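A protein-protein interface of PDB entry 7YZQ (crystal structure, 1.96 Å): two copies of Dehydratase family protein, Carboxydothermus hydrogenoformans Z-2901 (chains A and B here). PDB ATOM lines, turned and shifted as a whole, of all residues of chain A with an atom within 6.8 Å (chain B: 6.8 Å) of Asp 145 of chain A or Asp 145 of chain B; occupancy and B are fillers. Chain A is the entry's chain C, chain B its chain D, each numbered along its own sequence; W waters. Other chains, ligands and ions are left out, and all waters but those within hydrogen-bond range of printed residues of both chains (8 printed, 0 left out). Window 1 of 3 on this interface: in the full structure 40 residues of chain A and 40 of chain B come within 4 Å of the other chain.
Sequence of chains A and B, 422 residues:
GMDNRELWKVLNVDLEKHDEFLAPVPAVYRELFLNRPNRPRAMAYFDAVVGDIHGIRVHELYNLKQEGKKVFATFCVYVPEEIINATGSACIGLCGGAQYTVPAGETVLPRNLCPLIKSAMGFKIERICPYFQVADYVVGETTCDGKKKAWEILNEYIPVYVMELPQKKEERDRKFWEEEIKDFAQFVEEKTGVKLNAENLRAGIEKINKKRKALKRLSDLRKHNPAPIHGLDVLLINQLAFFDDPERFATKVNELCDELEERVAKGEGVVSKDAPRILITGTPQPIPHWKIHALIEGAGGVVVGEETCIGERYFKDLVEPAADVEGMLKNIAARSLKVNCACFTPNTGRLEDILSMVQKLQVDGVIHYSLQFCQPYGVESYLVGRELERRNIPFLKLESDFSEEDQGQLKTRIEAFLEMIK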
ATOM      1  N   LEU A 113     -17.711 -12.595 -16.374  1.00  0.00           N
ATOM      2  CA  LEU A 113     -18.166 -13.856 -15.794  1.00  0.00           C
ATOM      3  C   LEU A 113     -19.610 -13.664 -15.393  1.00  0.00           C
ATOM      4  O   LEU A 113     -20.068 -12.527 -15.228  1.00  0.00           O
ATOM      5  CB  LEU A 113     -17.321 -14.272 -14.567  1.00  0.00           C
ATOM      6  CG  LEU A 113     -17.183 -15.753 -14.291  1.00  0.00           C
ATOM      7  CD1 LEU A 113     -16.239 -16.401 -15.258  1.00  0.00           C
ATOM      8  CD2 LEU A 113     -16.761 -15.998 -12.819  1.00  0.00           C
ATOM      9  N   ILE A 117     -22.249 -15.968 -10.189  1.00  0.00           N
ATOM     10  CA  ILE A 117     -21.043 -16.430  -9.522  1.00  0.00           C
ATOM     11  C   ILE A 117     -20.353 -15.273  -8.802  1.00  0.00           C
ATOM     12  O   ILE A 117     -19.889 -15.394  -7.660  1.00  0.00           O
ATOM     13  CB  ILE A 117     -20.103 -17.082 -10.553  1.00  0.00           C
ATOM     14  CG1 ILE A 117     -20.813 -18.117 -11.427  1.00  0.00           C
ATOM     15  CG2 ILE A 117     -18.927 -17.731  -9.791  1.00  0.00           C
ATOM     16  CD1 ILE A 117     -19.925 -18.620 -12.594  1.00  0.00           C
ATOM     17  N   THR A 142     -19.219 -29.468 -10.655  1.00  0.00           N
ATOM     18  CA  THR A 142     -18.491 -29.197 -11.888  1.00  0.00           C
ATOM     19  C   THR A 142     -19.457 -29.031 -13.057  1.00  0.00           C
ATOM     20  O   THR A 142     -19.617 -29.894 -13.908  1.00  0.00           O
ATOM     21  CB  THR A 142     -17.486 -30.309 -12.162  1.00  0.00           C
ATOM     22  OG1 THR A 142     -18.121 -31.589 -12.153  1.00  0.00           O
ATOM     23  CG2 THR A 142     -16.349 -30.284 -11.096  1.00  0.00           C
ATOM     24  N   THR A 143     -20.127 -27.895 -13.065  1.00  0.00           N
ATOM     25  CA  THR A 143     -21.041 -27.546 -14.141  1.00  0.00           C
ATOM     26  C   THR A 143     -20.385 -26.542 -15.067  1.00  0.00           C
ATOM     27  O   THR A 143     -19.630 -26.936 -15.967  1.00  0.00           O
ATOM     28  CB  THR A 143     -22.343 -26.947 -13.593  1.00  0.00           C
ATOM     29  OG1 THR A 143     -22.018 -26.058 -12.510  1.00  0.00           O
ATOM     30  CG2 THR A 143     -23.282 -28.028 -13.123  1.00  0.00           C
ATOM     31  N   CYS A 144     -20.657 -25.250 -14.912  1.00  0.00           N
ATOM     32  CA  CYS A 144     -20.131 -24.286 -15.851  1.00  0.00           C
ATOM     33  C   CYS A 144     -18.702 -23.971 -15.475  1.00  0.00           C
ATOM     34  O   CYS A 144     -18.169 -24.418 -14.424  1.00  0.00           O
ATOM     35  CB  CYS A 144     -20.963 -22.997 -15.824  1.00  0.00           C
ATOM     36  SG  CYS A 144     -20.861 -22.354 -14.072  1.00  0.00           S
ATOM     37  N   ASP A 145     -17.971 -23.371 -16.406  1.00  0.00           N
ATOM     38  CA  ASP A 145     -16.556 -23.128 -16.208  1.00  0.00           C
ATOM     39  C   ASP A 145     -16.323 -22.188 -15.028  1.00  0.00           C
ATOM     40  O   ASP A 145     -15.465 -22.443 -14.169  1.00  0.00           O
ATOM     41  CB  ASP A 145     -15.925 -22.538 -17.484  1.00  0.00           C
ATOM     42  CG  ASP A 145     -15.874 -23.505 -18.635  1.00  0.00           C
ATOM     43  OD1 ASP A 145     -15.941 -24.709 -18.386  1.00  0.00           O
ATOM     44  OD2 ASP A 145     -15.770 -23.056 -19.823  1.00  0.00           O
ATOM     45  N   GLY A 146     -17.133 -21.133 -14.937  1.00  0.00           N
ATOM     46  CA  GLY A 146     -16.919 -20.127 -13.924  1.00  0.00           C
ATOM     47  C   GLY A 146     -17.081 -20.683 -12.527  1.00  0.00           C
ATOM     48  O   GLY A 146     -16.314 -20.352 -11.640  1.00  0.00           O
ATOM     49  N   LYS A 147     -18.086 -21.529 -12.318  1.00  0.00           N
ATOM     50  CA  LYS A 147     -18.330 -22.131 -11.015  1.00  0.00           C
ATOM     51  C   LYS A 147     -17.220 -23.095 -10.661  1.00  0.00           C
ATOM     52  O   LYS A 147     -16.688 -23.056  -9.543  1.00  0.00           O
ATOM     53  CB  LYS A 147     -19.672 -22.870 -11.028  1.00  0.00           C
ATOM     54  CG  LYS A 147     -20.873 -22.102 -10.552  1.00  0.00           C
ATOM     55  CD  LYS A 147     -22.108 -22.976 -10.835  1.00  0.00           C
ATOM     56  CE  LYS A 147     -23.233 -22.537 -10.004  1.00  0.00           C
ATOM     57  NZ  LYS A 147     -24.425 -23.508 -10.217  1.00  0.00           N
ATOM     58  N   LYS A 148     -16.892 -24.001 -11.596  1.00  0.00           N
ATOM     59  CA  LYS A 148     -15.851 -25.000 -11.348  1.00  0.00           C
ATOM     60  C   LYS A 148     -14.565 -24.340 -10.838  1.00  0.00           C
ATOM     61  O   LYS A 148     -13.968 -24.760  -9.833  1.00  0.00           O
ATOM     62  CB  LYS A 148     -15.590 -25.828 -12.626  1.00  0.00           C
ATOM     63  CG  LYS A 148     -14.472 -26.856 -12.499  1.00  0.00           C
ATOM     64  CD  LYS A 148     -14.460 -27.834 -13.638  1.00  0.00           C
ATOM     65  CE  LYS A 148     -14.356 -27.127 -14.985  1.00  0.00           C
ATOM     66  NZ  LYS A 148     -14.087 -28.099 -16.075  1.00  0.00           N
ATOM     67  N   LYS A 149     -14.127 -23.312 -11.538  1.00  0.00           N
ATOM     68  CA  LYS A 149     -12.886 -22.652 -11.186  1.00  0.00           C
ATOM     69  C   LYS A 149     -13.066 -21.707  -9.999  1.00  0.00           C
ATOM     70  O   LYS A 149     -12.110 -21.485  -9.254  1.00  0.00           O
ATOM     71  CB  LYS A 149     -12.345 -21.896 -12.411  1.00  0.00           C
ATOM     72  CG  LYS A 149     -12.122 -22.781 -13.630  1.00  0.00           C
ATOM     73  CD  LYS A 149     -11.262 -24.001 -13.356  1.00  0.00           C
ATOM     74  CE  LYS A 149      -9.756 -23.581 -13.233  1.00  0.00           C
ATOM     75  NZ  LYS A 149      -8.941 -24.793 -13.031  1.00  0.00           N
ATOM     76  N   ALA A 150     -14.274 -21.166  -9.793  1.00  0.00           N
ATOM     77  CA  ALA A 150     -14.532 -20.346  -8.618  1.00  0.00           C
ATOM     78  C   ALA A 150     -14.395 -21.157  -7.344  1.00  0.00           C
ATOM     79  O   ALA A 150     -13.887 -20.650  -6.341  1.00  0.00           O
ATOM     80  CB  ALA A 150     -15.928 -19.726  -8.681  1.00  0.00           C
ATOM     81  N   GLN A 167     -20.893 -34.815 -18.080  1.00  0.00           N
ATOM     82  CA  GLN A 167     -21.345 -33.916 -19.137  1.00  0.00           C
ATOM     83  C   GLN A 167     -22.226 -34.578 -20.181  1.00  0.00           C
ATOM     84  O   GLN A 167     -22.730 -33.882 -21.075  1.00  0.00           O
ATOM     85  CB  GLN A 167     -20.125 -33.292 -19.810  1.00  0.00           C
ATOM     86  CG  GLN A 167     -19.140 -32.761 -18.767  1.00  0.00           C
ATOM     87  CD  GLN A 167     -17.976 -32.007 -19.370  1.00  0.00           C
ATOM     88  OE1 GLN A 167     -18.155 -31.014 -20.047  1.00  0.00           O
ATOM     89  NE2 GLN A 167     -16.768 -32.451 -19.069  1.00  0.00           N
ATOM     90  N   ALA A 342     -28.102 -27.087 -19.453  1.00  0.00           N
ATOM     91  CA  ALA A 342     -27.310 -26.874 -20.670  1.00  0.00           C
ATOM     92  C   ALA A 342     -25.852 -27.258 -20.518  1.00  0.00           C
ATOM     93  O   ALA A 342     -25.123 -27.296 -21.526  1.00  0.00           O
ATOM     94  CB  ALA A 342     -27.433 -25.382 -21.145  1.00  0.00           C
ATOM     95  N   CYS A 343     -25.410 -27.594 -19.306  1.00  0.00           N
ATOM     96  CA  CYS A 343     -24.050 -28.108 -19.137  1.00  0.00           C
ATOM     97  C   CYS A 343     -23.917 -29.547 -19.627  1.00  0.00           C
ATOM     98  O   CYS A 343     -22.802 -30.019 -19.835  1.00  0.00           O
ATOM     99  CB  CYS A 343     -23.604 -27.983 -17.667  1.00  0.00           C
ATOM    100  SG  CYS A 343     -23.489 -26.298 -17.066  1.00  0.00           S
ATOM    101  N   PHE A 373     -22.710 -13.559 -19.949  1.00  0.00           N
ATOM    102  CA  PHE A 373     -21.539 -14.426 -19.885  1.00  0.00           C
ATOM    103  C   PHE A 373     -21.860 -15.828 -19.383  1.00  0.00           C
ATOM    104  O   PHE A 373     -20.917 -16.573 -19.022  1.00  0.00           O
ATOM    105  CB  PHE A 373     -20.421 -13.812 -19.020  1.00  0.00           C
ATOM    106  CG  PHE A 373     -20.019 -12.466 -19.474  1.00  0.00           C
ATOM    107  CD1 PHE A 373     -19.391 -12.303 -20.697  1.00  0.00           C
ATOM    108  CD2 PHE A 373     -20.293 -11.362 -18.719  1.00  0.00           C
ATOM    109  CE1 PHE A 373     -19.059 -11.044 -21.154  1.00  0.00           C
ATOM    110  CE2 PHE A 373     -19.942 -10.106 -19.173  1.00  0.00           C
ATOM    111  CZ  PHE A 373     -19.358  -9.958 -20.403  1.00  0.00           C
ATOM    112  N   CYS A 374     -23.139 -16.234 -19.352  1.00  0.00           N
ATOM    113  CA  CYS A 374     -23.447 -17.638 -19.100  1.00  0.00           C
ATOM    114  C   CYS A 374     -23.330 -18.302 -20.457  1.00  0.00           C
ATOM    115  O   CYS A 374     -24.202 -18.137 -21.326  1.00  0.00           O
ATOM    116  CB  CYS A 374     -24.826 -17.875 -18.518  1.00  0.00           C
ATOM    117  SG  CYS A 374     -25.244 -19.671 -18.576  1.00  0.00           S
ATOM    118  N   GLN A 375     -22.257 -19.012 -20.672  1.00  0.00           N
ATOM    119  CA  GLN A 375     -21.992 -19.538 -22.003  1.00  0.00           C
ATOM    120  C   GLN A 375     -22.784 -20.813 -22.284  1.00  0.00           C
ATOM    121  O   GLN A 375     -23.243 -21.001 -23.419  1.00  0.00           O
ATOM    122  CB  GLN A 375     -20.488 -19.788 -22.189  1.00  0.00           C
ATOM    123  CG  GLN A 375     -19.606 -18.663 -21.699  1.00  0.00           C
ATOM    124  CD  GLN A 375     -19.628 -17.411 -22.569  1.00  0.00           C
ATOM    125  OE1 GLN A 375     -20.686 -16.819 -22.849  1.00  0.00           O
ATOM    126  NE2 GLN A 375     -18.436 -16.968 -22.972  1.00  0.00           N
ATOM    127  N   PRO A 376     -22.989 -21.710 -21.301  1.00  0.00           N
ATOM    128  CA  PRO A 376     -23.852 -22.879 -21.585  1.00  0.00           C
ATOM    129  C   PRO A 376     -25.234 -22.485 -22.115  1.00  0.00           C
ATOM    130  O   PRO A 376     -25.656 -22.991 -23.178  1.00  0.00           O
ATOM    131  CB  PRO A 376     -23.893 -23.626 -20.242  1.00  0.00           C
ATOM    132  CG  PRO A 376     -22.596 -23.236 -19.556  1.00  0.00           C
ATOM    133  CD  PRO A 376     -22.315 -21.827 -19.991  1.00  0.00           C
ATOM    134  N   VAL A 379     -24.967 -20.097 -25.528  1.00  0.00           N
ATOM    135  CA  VAL A 379     -24.716 -20.792 -26.786  1.00  0.00           C
ATOM    136  C   VAL A 379     -25.919 -21.634 -27.165  1.00  0.00           C
ATOM    137  O   VAL A 379     -26.349 -21.652 -28.327  1.00  0.00           O
ATOM    138  CB  VAL A 379     -23.446 -21.647 -26.694  1.00  0.00           C
ATOM    139  CG1 VAL A 379     -23.279 -22.506 -27.992  1.00  0.00           C
ATOM    140  CG2 VAL A 379     -22.176 -20.779 -26.511  1.00  0.00           C
ATOM    141  N   LEU B 113     -17.898 -14.610 -26.743  1.00  0.00           N
ATOM    142  CA  LEU B 113     -17.403 -15.975 -26.616  1.00  0.00           C
ATOM    143  C   LEU B 113     -15.953 -15.967 -27.101  1.00  0.00           C
ATOM    144  O   LEU B 113     -15.545 -15.086 -27.865  1.00  0.00           O
ATOM    145  CB  LEU B 113     -18.237 -16.944 -27.446  1.00  0.00           C
ATOM    146  CG  LEU B 113     -18.071 -18.414 -27.115  1.00  0.00           C
ATOM    147  CD1 LEU B 113     -18.943 -18.826 -25.919  1.00  0.00           C
ATOM    148  CD2 LEU B 113     -18.431 -19.273 -28.301  1.00  0.00           C
ATOM    149  N   ILE B 117     -12.956 -20.174 -30.817  1.00  0.00           N
ATOM    150  CA  ILE B 117     -14.167 -20.903 -31.217  1.00  0.00           C
ATOM    151  C   ILE B 117     -14.915 -20.194 -32.351  1.00  0.00           C
ATOM    152  O   ILE B 117     -15.270 -20.803 -33.374  1.00  0.00           O
ATOM    153  CB  ILE B 117     -15.087 -21.072 -29.992  1.00  0.00           C
ATOM    154  CG1 ILE B 117     -14.324 -21.728 -28.849  1.00  0.00           C
ATOM    155  CG2 ILE B 117     -16.308 -21.903 -30.387  1.00  0.00           C
ATOM    156  CD1 ILE B 117     -15.006 -21.573 -27.470  1.00  0.00           C
ATOM    157  N   THR B 142     -15.237 -32.366 -24.623  1.00  0.00           N
ATOM    158  CA  THR B 142     -16.010 -31.647 -23.599  1.00  0.00           C
ATOM    159  C   THR B 142     -15.052 -30.956 -22.621  1.00  0.00           C
ATOM    160  O   THR B 142     -14.889 -31.355 -21.450  1.00  0.00           O
ATOM    161  CB  THR B 142     -16.955 -32.588 -22.851  1.00  0.00           C
ATOM    162  OG1 THR B 142     -16.238 -33.689 -22.234  1.00  0.00           O
ATOM    163  CG2 THR B 142     -18.013 -33.211 -23.771  1.00  0.00           C
ATOM    164  N   THR B 143     -14.396 -29.906 -23.135  1.00  0.00           N
ATOM    165  CA  THR B 143     -13.508 -29.080 -22.319  1.00  0.00           C
ATOM    166  C   THR B 143     -14.217 -27.826 -21.812  1.00  0.00           C
ATOM    167  O   THR B 143     -14.914 -27.885 -20.792  1.00  0.00           O
ATOM    168  CB  THR B 143     -12.251 -28.710 -23.099  1.00  0.00           C
ATOM    169  OG1 THR B 143     -12.614 -28.404 -24.425  1.00  0.00           O
ATOM    170  CG2 THR B 143     -11.247 -29.893 -23.113  1.00  0.00           C
ATOM    171  N   CYS B 144     -14.058 -26.687 -22.497  1.00  0.00           N
ATOM    172  CA  CYS B 144     -14.717 -25.484 -22.018  1.00  0.00           C
ATOM    173  C   CYS B 144     -16.172 -25.441 -22.505  1.00  0.00           C
ATOM    174  O   CYS B 144     -16.584 -26.186 -23.396  1.00  0.00           O
ATOM    175  CB  CYS B 144     -13.972 -24.239 -22.485  1.00  0.00           C
ATOM    176  SG  CYS B 144     -13.974 -24.124 -24.298  1.00  0.00           S
ATOM    177  N   ASP B 145     -16.951 -24.563 -21.874  1.00  0.00           N
ATOM    178  CA  ASP B 145     -18.377 -24.432 -22.163  1.00  0.00           C
ATOM    179  C   ASP B 145     -18.624 -24.084 -23.618  1.00  0.00           C
ATOM    180  O   ASP B 145     -19.522 -24.642 -24.269  1.00  0.00           O
ATOM    181  CB  ASP B 145     -18.978 -23.343 -21.270  1.00  0.00           C
ATOM    182  CG  ASP B 145     -18.995 -23.706 -19.799  1.00  0.00           C
ATOM    183  OD1 ASP B 145     -18.988 -24.918 -19.430  1.00  0.00           O
ATOM    184  OD2 ASP B 145     -19.096 -22.739 -19.013  1.00  0.00           O
ATOM    185  N   GLY B 146     -17.870 -23.119 -24.129  1.00  0.00           N
ATOM    186  CA  GLY B 146     -18.114 -22.655 -25.474  1.00  0.00           C
ATOM    187  C   GLY B 146     -17.884 -23.746 -26.501  1.00  0.00           C
ATOM    188  O   GLY B 146     -18.660 -23.880 -27.446  1.00  0.00           O
ATOM    189  N   LYS B 147     -16.799 -24.529 -26.342  1.00  0.00           N
ATOM    190  CA  LYS B 147     -16.494 -25.580 -27.312  1.00  0.00           C
ATOM    191  C   LYS B 147     -17.527 -26.685 -27.246  1.00  0.00           C
ATOM    192  O   LYS B 147     -18.032 -27.150 -28.278  1.00  0.00           O
ATOM    193  CB  LYS B 147     -15.115 -26.186 -27.061  1.00  0.00           C
ATOM    194  CG  LYS B 147     -13.953 -25.480 -27.745  1.00  0.00           C
ATOM    195  CD  LYS B 147     -12.643 -26.012 -27.146  1.00  0.00           C
ATOM    196  CE  LYS B 147     -11.589 -26.262 -28.160  1.00  0.00           C
ATOM    197  NZ  LYS B 147     -10.316 -26.656 -27.482  1.00  0.00           N
ATOM    198  N   LYS B 148     -17.834 -27.127 -26.033  1.00  0.00           N
ATOM    199  CA  LYS B 148     -18.787 -28.218 -25.869  1.00  0.00           C
ATOM    200  C   LYS B 148     -20.129 -27.865 -26.498  1.00  0.00           C
ATOM    201  O   LYS B 148     -20.742 -28.702 -27.160  1.00  0.00           O
ATOM    202  CB  LYS B 148     -18.972 -28.551 -24.387  1.00  0.00           C
ATOM    203  CG  LYS B 148     -20.190 -29.464 -24.111  1.00  0.00           C
ATOM    204  CD  LYS B 148     -20.263 -29.900 -22.658  1.00  0.00           C
ATOM    205  CE  LYS B 148     -20.354 -28.707 -21.690  1.00  0.00           C
ATOM    206  NZ  LYS B 148     -20.452 -29.196 -20.251  1.00  0.00           N
ATOM    207  N   LYS B 149     -20.626 -26.644 -26.284  1.00  0.00           N
ATOM    208  CA  LYS B 149     -21.927 -26.297 -26.847  1.00  0.00           C
ATOM    209  C   LYS B 149     -21.828 -25.964 -28.347  1.00  0.00           C
ATOM    210  O   LYS B 149     -22.789 -26.154 -29.109  1.00  0.00           O
ATOM    211  CB  LYS B 149     -22.519 -25.123 -26.057  1.00  0.00           C
ATOM    212  CG  LYS B 149     -22.799 -25.380 -24.582  1.00  0.00           C
ATOM    213  CD  LYS B 149     -23.530 -26.673 -24.283  1.00  0.00           C
ATOM    214  CE  LYS B 149     -24.999 -26.579 -24.591  1.00  0.00           C
ATOM    215  NZ  LYS B 149     -25.744 -27.846 -24.379  1.00  0.00           N
ATOM    216  N   ALA B 150     -20.676 -25.470 -28.792  1.00  0.00           N
ATOM    217  CA  ALA B 150     -20.487 -25.185 -30.213  1.00  0.00           C
ATOM    218  C   ALA B 150     -20.525 -26.458 -31.040  1.00  0.00           C
ATOM    219  O   ALA B 150     -20.994 -26.429 -32.188  1.00  0.00           O
ATOM    220  CB  ALA B 150     -19.146 -24.477 -30.477  1.00  0.00           C
ATOM    221  N   GLN B 167     -13.398 -34.207 -15.513  1.00  0.00           N
ATOM    222  CA  GLN B 167     -13.038 -32.882 -15.017  1.00  0.00           C
ATOM    223  C   GLN B 167     -12.117 -32.934 -13.797  1.00  0.00           C
ATOM    224  O   GLN B 167     -11.752 -31.876 -13.262  1.00  0.00           O
ATOM    225  CB  GLN B 167     -14.302 -32.055 -14.701  1.00  0.00           C
ATOM    226  CG  GLN B 167     -15.154 -31.757 -15.924  1.00  0.00           C
ATOM    227  CD  GLN B 167     -16.401 -31.005 -15.612  1.00  0.00           C
ATOM    228  OE1 GLN B 167     -16.386 -29.769 -15.485  1.00  0.00           O
ATOM    229  NE2 GLN B 167     -17.505 -31.727 -15.506  1.00  0.00           N
ATOM    230  N   CYS B 343      -9.195 -26.744 -17.644  1.00  0.00           N
ATOM    231  CA  CYS B 343     -10.504 -27.376 -17.554  1.00  0.00           C
ATOM    232  C   CYS B 343     -10.560 -28.439 -16.459  1.00  0.00           C
ATOM    233  O   CYS B 343     -11.643 -28.926 -16.142  1.00  0.00           O
ATOM    234  CB  CYS B 343     -10.869 -27.959 -18.928  1.00  0.00           C
ATOM    235  SG  CYS B 343     -11.301 -26.651 -20.105  1.00  0.00           S
ATOM    236  N   PHE B 373     -12.662 -13.779 -22.987  1.00  0.00           N
ATOM    237  CA  PHE B 373     -13.811 -14.655 -22.737  1.00  0.00           C
ATOM    238  C   PHE B 373     -13.409 -16.111 -22.561  1.00  0.00           C
ATOM    239  O   PHE B 373     -14.283 -16.995 -22.464  1.00  0.00           O
ATOM    240  CB  PHE B 373     -14.848 -14.498 -23.856  1.00  0.00           C
ATOM    241  CG  PHE B 373     -15.203 -13.060 -24.129  1.00  0.00           C
ATOM    242  CD1 PHE B 373     -15.703 -12.268 -23.129  1.00  0.00           C
ATOM    243  CD2 PHE B 373     -15.065 -12.514 -25.388  1.00  0.00           C
ATOM    244  CE1 PHE B 373     -16.034 -10.955 -23.364  1.00  0.00           C
ATOM    245  CE2 PHE B 373     -15.408 -11.192 -25.649  1.00  0.00           C
ATOM    246  CZ  PHE B 373     -15.875 -10.396 -24.629  1.00  0.00           C
ATOM    247  N   CYS B 374     -12.110 -16.393 -22.474  1.00  0.00           N
ATOM    248  CA  CYS B 374     -11.663 -17.721 -22.050  1.00  0.00           C
ATOM    249  C   CYS B 374     -11.824 -17.820 -20.533  1.00  0.00           C
ATOM    250  O   CYS B 374     -11.011 -17.292 -19.765  1.00  0.00           O
ATOM    251  CB  CYS B 374     -10.207 -18.011 -22.393  1.00  0.00           C
ATOM    252  SG  CYS B 374      -9.766 -19.661 -21.682  1.00  0.00           S
ATOM    253  N   GLN B 375     -12.851 -18.504 -20.089  1.00  0.00           N
ATOM    254  CA  GLN B 375     -13.146 -18.453 -18.670  1.00  0.00           C
ATOM    255  C   GLN B 375     -12.304 -19.435 -17.866  1.00  0.00           C
ATOM    256  O   GLN B 375     -11.863 -19.086 -16.762  1.00  0.00           O
ATOM    257  CB  GLN B 375     -14.653 -18.669 -18.514  1.00  0.00           C
ATOM    258  CG  GLN B 375     -15.434 -17.505 -19.149  1.00  0.00           C
ATOM    259  CD  GLN B 375     -16.949 -17.669 -19.064  1.00  0.00           C
ATOM    260  OE1 GLN B 375     -17.463 -18.768 -19.217  1.00  0.00           O
ATOM    261  NE2 GLN B 375     -17.664 -16.569 -18.845  1.00  0.00           N
ATOM    262  N   PRO B 376     -12.015 -20.641 -18.361  1.00  0.00           N
ATOM    263  CA  PRO B 376     -11.163 -21.523 -17.550  1.00  0.00           C
ATOM    264  C   PRO B 376      -9.822 -20.881 -17.220  1.00  0.00           C
ATOM    265  O   PRO B 376      -9.394 -20.863 -16.053  1.00  0.00           O
ATOM    266  CB  PRO B 376     -11.017 -22.775 -18.424  1.00  0.00           C
ATOM    267  CG  PRO B 376     -12.254 -22.794 -19.264  1.00  0.00           C
ATOM    268  CD  PRO B 376     -12.559 -21.338 -19.539  1.00  0.00           C
ATOM    269  N   VAL B 379     -10.187 -17.427 -15.136  1.00  0.00           N
ATOM    270  CA  VAL B 379     -10.390 -17.553 -13.699  1.00  0.00           C
ATOM    271  C   VAL B 379      -9.129 -18.070 -13.030  1.00  0.00           C
ATOM    272  O   VAL B 379      -8.715 -17.555 -11.985  1.00  0.00           O
ATOM    273  CB  VAL B 379     -11.595 -18.458 -13.397  1.00  0.00           C
ATOM    274  CG1 VAL B 379     -11.794 -18.606 -11.877  1.00  0.00           C
ATOM    275  CG2 VAL B 379     -12.848 -17.866 -14.005  1.00  0.00           C
HETATM  276  O   HOH W   1     -15.770 -20.516 -20.974  1.00  0.00           O
HETATM  277  O   HOH W   2     -19.444 -17.225 -16.638  1.00  0.00           O
HETATM  278  O   HOH W   3     -14.041 -26.676 -18.467  1.00  0.00           O
HETATM  279  O   HOH W   4     -19.578 -20.273 -18.934  1.00  0.00           O
HETATM  280  O   HOH W   5     -17.486 -28.909 -18.031  1.00  0.00           O
HETATM  281  O   HOH W   6     -19.891 -29.570 -17.200  1.00  0.00           O
HETATM  282  O   HOH W   7     -14.707 -29.924 -18.806  1.00  0.00           O
HETATM  283  O   HOH W   8     -20.665 -26.731 -18.611  1.00  0.00           O
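The side-chain sulfur (SG) of Cys 343 of chain A lies within hydrogen-bond range of the backbone NH (N) of Cys 144 of chain A, at 3.7 Å.
The backbone NH (N) of Lys 147 of chain B lies close to the side-chain sulfur (SG) of Cys 144 of chain B.
N of Cys 144 of chain B is in hydrogen-bond range of SG of Cys 343 of chain B (3.7 Å).
N of Lys 147 of chain A lies close to SG of Cys 144 of chain A, at 3.4 Å.
Printed residues of chain B within 4 Å of Leu 113 of chain A: Gln 375 and Val 379.
Asp 145 of chain A touches just these residues of chain B: Cys 144, Asp 145 and Pro 376.
Gly 146 of chain A touches none of the printed residues of chain B.
Of the printed residues of chain B, Ala 342 of chain A touches Lys 149.
Of the printed residues of chain A, Asp 145 of chain B touches Cys 144 (3.7 Å), Asp 145 (2.8 Å), Gln 375 (3.97 Å) and Pro 376 (3.5 Å).
The side-chain amide nitrogen (NE2) of Gln 167 of chain A lies within hydrogen-bond range of the backbone carbonyl oxygen (O) of Thr 142 of chain B (3.2 Å).
NZ of Lys 148 of chain B lies within hydrogen-bond range of O of Cys 343 of chain A (2.5 Å).
The side-chain amide oxygen (OE1) of Gln 167 of chain B is in hydrogen-bond range of the side-chain amino group (NZ) of Lys 148 of chain A (2.9 Å).
N of Asp 145 of chain B lies within hydrogen-bond range of OD2 of Asp 145 of chain A (2.8 Å).
The backbone carbonyl oxygen (O) of Cys 343 of chain B is in hydrogen-bond range of the side-chain amino group (NZ) of Lys 148 of chain A, 2.6 Å away.
The side-chain amide oxygen of Gln 167 of chain A sits at hydrogen-bond distance from the side-chain amino group of Lys 148 of chain B, at 2.9 Å.
The side-chain amide nitrogen (NE2) of Gln 167 of chain B sits at hydrogen-bond distance from the backbone carbonyl oxygen (O) of Thr 142 of chain A (3.2 Å).
The backbone carbonyl oxygen (O) of Phe 373 of chain A sits at hydrogen-bond distance from the side-chain amide nitrogen (NE2) of Gln 375 of chain B, at 3.3 Å.
O of Ala 342 of chain A is in hydrogen-bond range of NZ of Lys 149 of chain B.
Water W8 lies within hydrogen-bond range of OD1 of Asp 145 of chain B (2.6 Å), O of Thr 143 of chain A (2.8 Å), NZ of Lys 148 of chain B (3.0 Å) and SG of Cys 343 of chain A (3.2 Å).
Water W6 lies within hydrogen-bond range of the backbone carbonyl oxygen of Thr 143 of chain A (2.9 Å), the side-chain amino group of Lys 148 of chain B (3.1 Å) and the backbone carbonyl oxygen of Thr 142 of chain A (3.3 Å).
Leu 113 of chain A touches Gln 375 of chain B, and with the chains exchanged Gln 375 of chain A touches Leu 113 of chain B.
Leu 113 of chain A touches Val 379 of chain B, and with the chains exchanged Val 379 of chain A touches Leu 113 of chain B.
Of the 25 pairs that touch across the chains among the printed residues, 22 have their exchanged pair printed and touching as well.
Of the 18 printed residues of chain B, 12 touch a printed residue of chain A.
Printed residues of chain B that touch a printed residue of chain A: Leu 113, Thr 142, Cys 144, Asp 145, Lys 148, Lys 149, Gln 167, Cys 343, Phe 373, Gln 375, Pro 376 and Val 379.
Hydrophobic or aromatic side chains of chain A within 4 Å of the printed part of chain B: Leu 113, Phe 373, Pro 376 and Val 379.
Among the printed residues, 25 pairs touch across the chains.
Among the printed residues, pairs that only touch across the chains: Gln 375 of chain A with Gln 375 of chain B, Val 379 of chain A with Lys 149 of chain B, Lys 149 of chain A with Val 379 of chain B, Asp 145 of chain A with Cys 144 of chain B, Pro 376 of chain A with Asp 145 of chain B, Gln 375 of chain A with Leu 113 of chain B, Asp 145 of chain A with Pro 376 of chain B, Gln 167 of chain A with Gln 167 of chain B, Cys 144 of chain A with Asp 145 of chain B, Phe 373 of chain A with Phe 373 of chain B, Val 379 of chain A with Leu 113 of chain B, Leu 113 of chain A with Gln 375 of chain B, Leu 113 of chain A with Val 379 of chain B, Pro 376 of chain A with Lys 149 of chain B, Lys 149 of chain A with Pro 376 of chain B and Gln 375 of chain A with Asp 145 of chain B.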
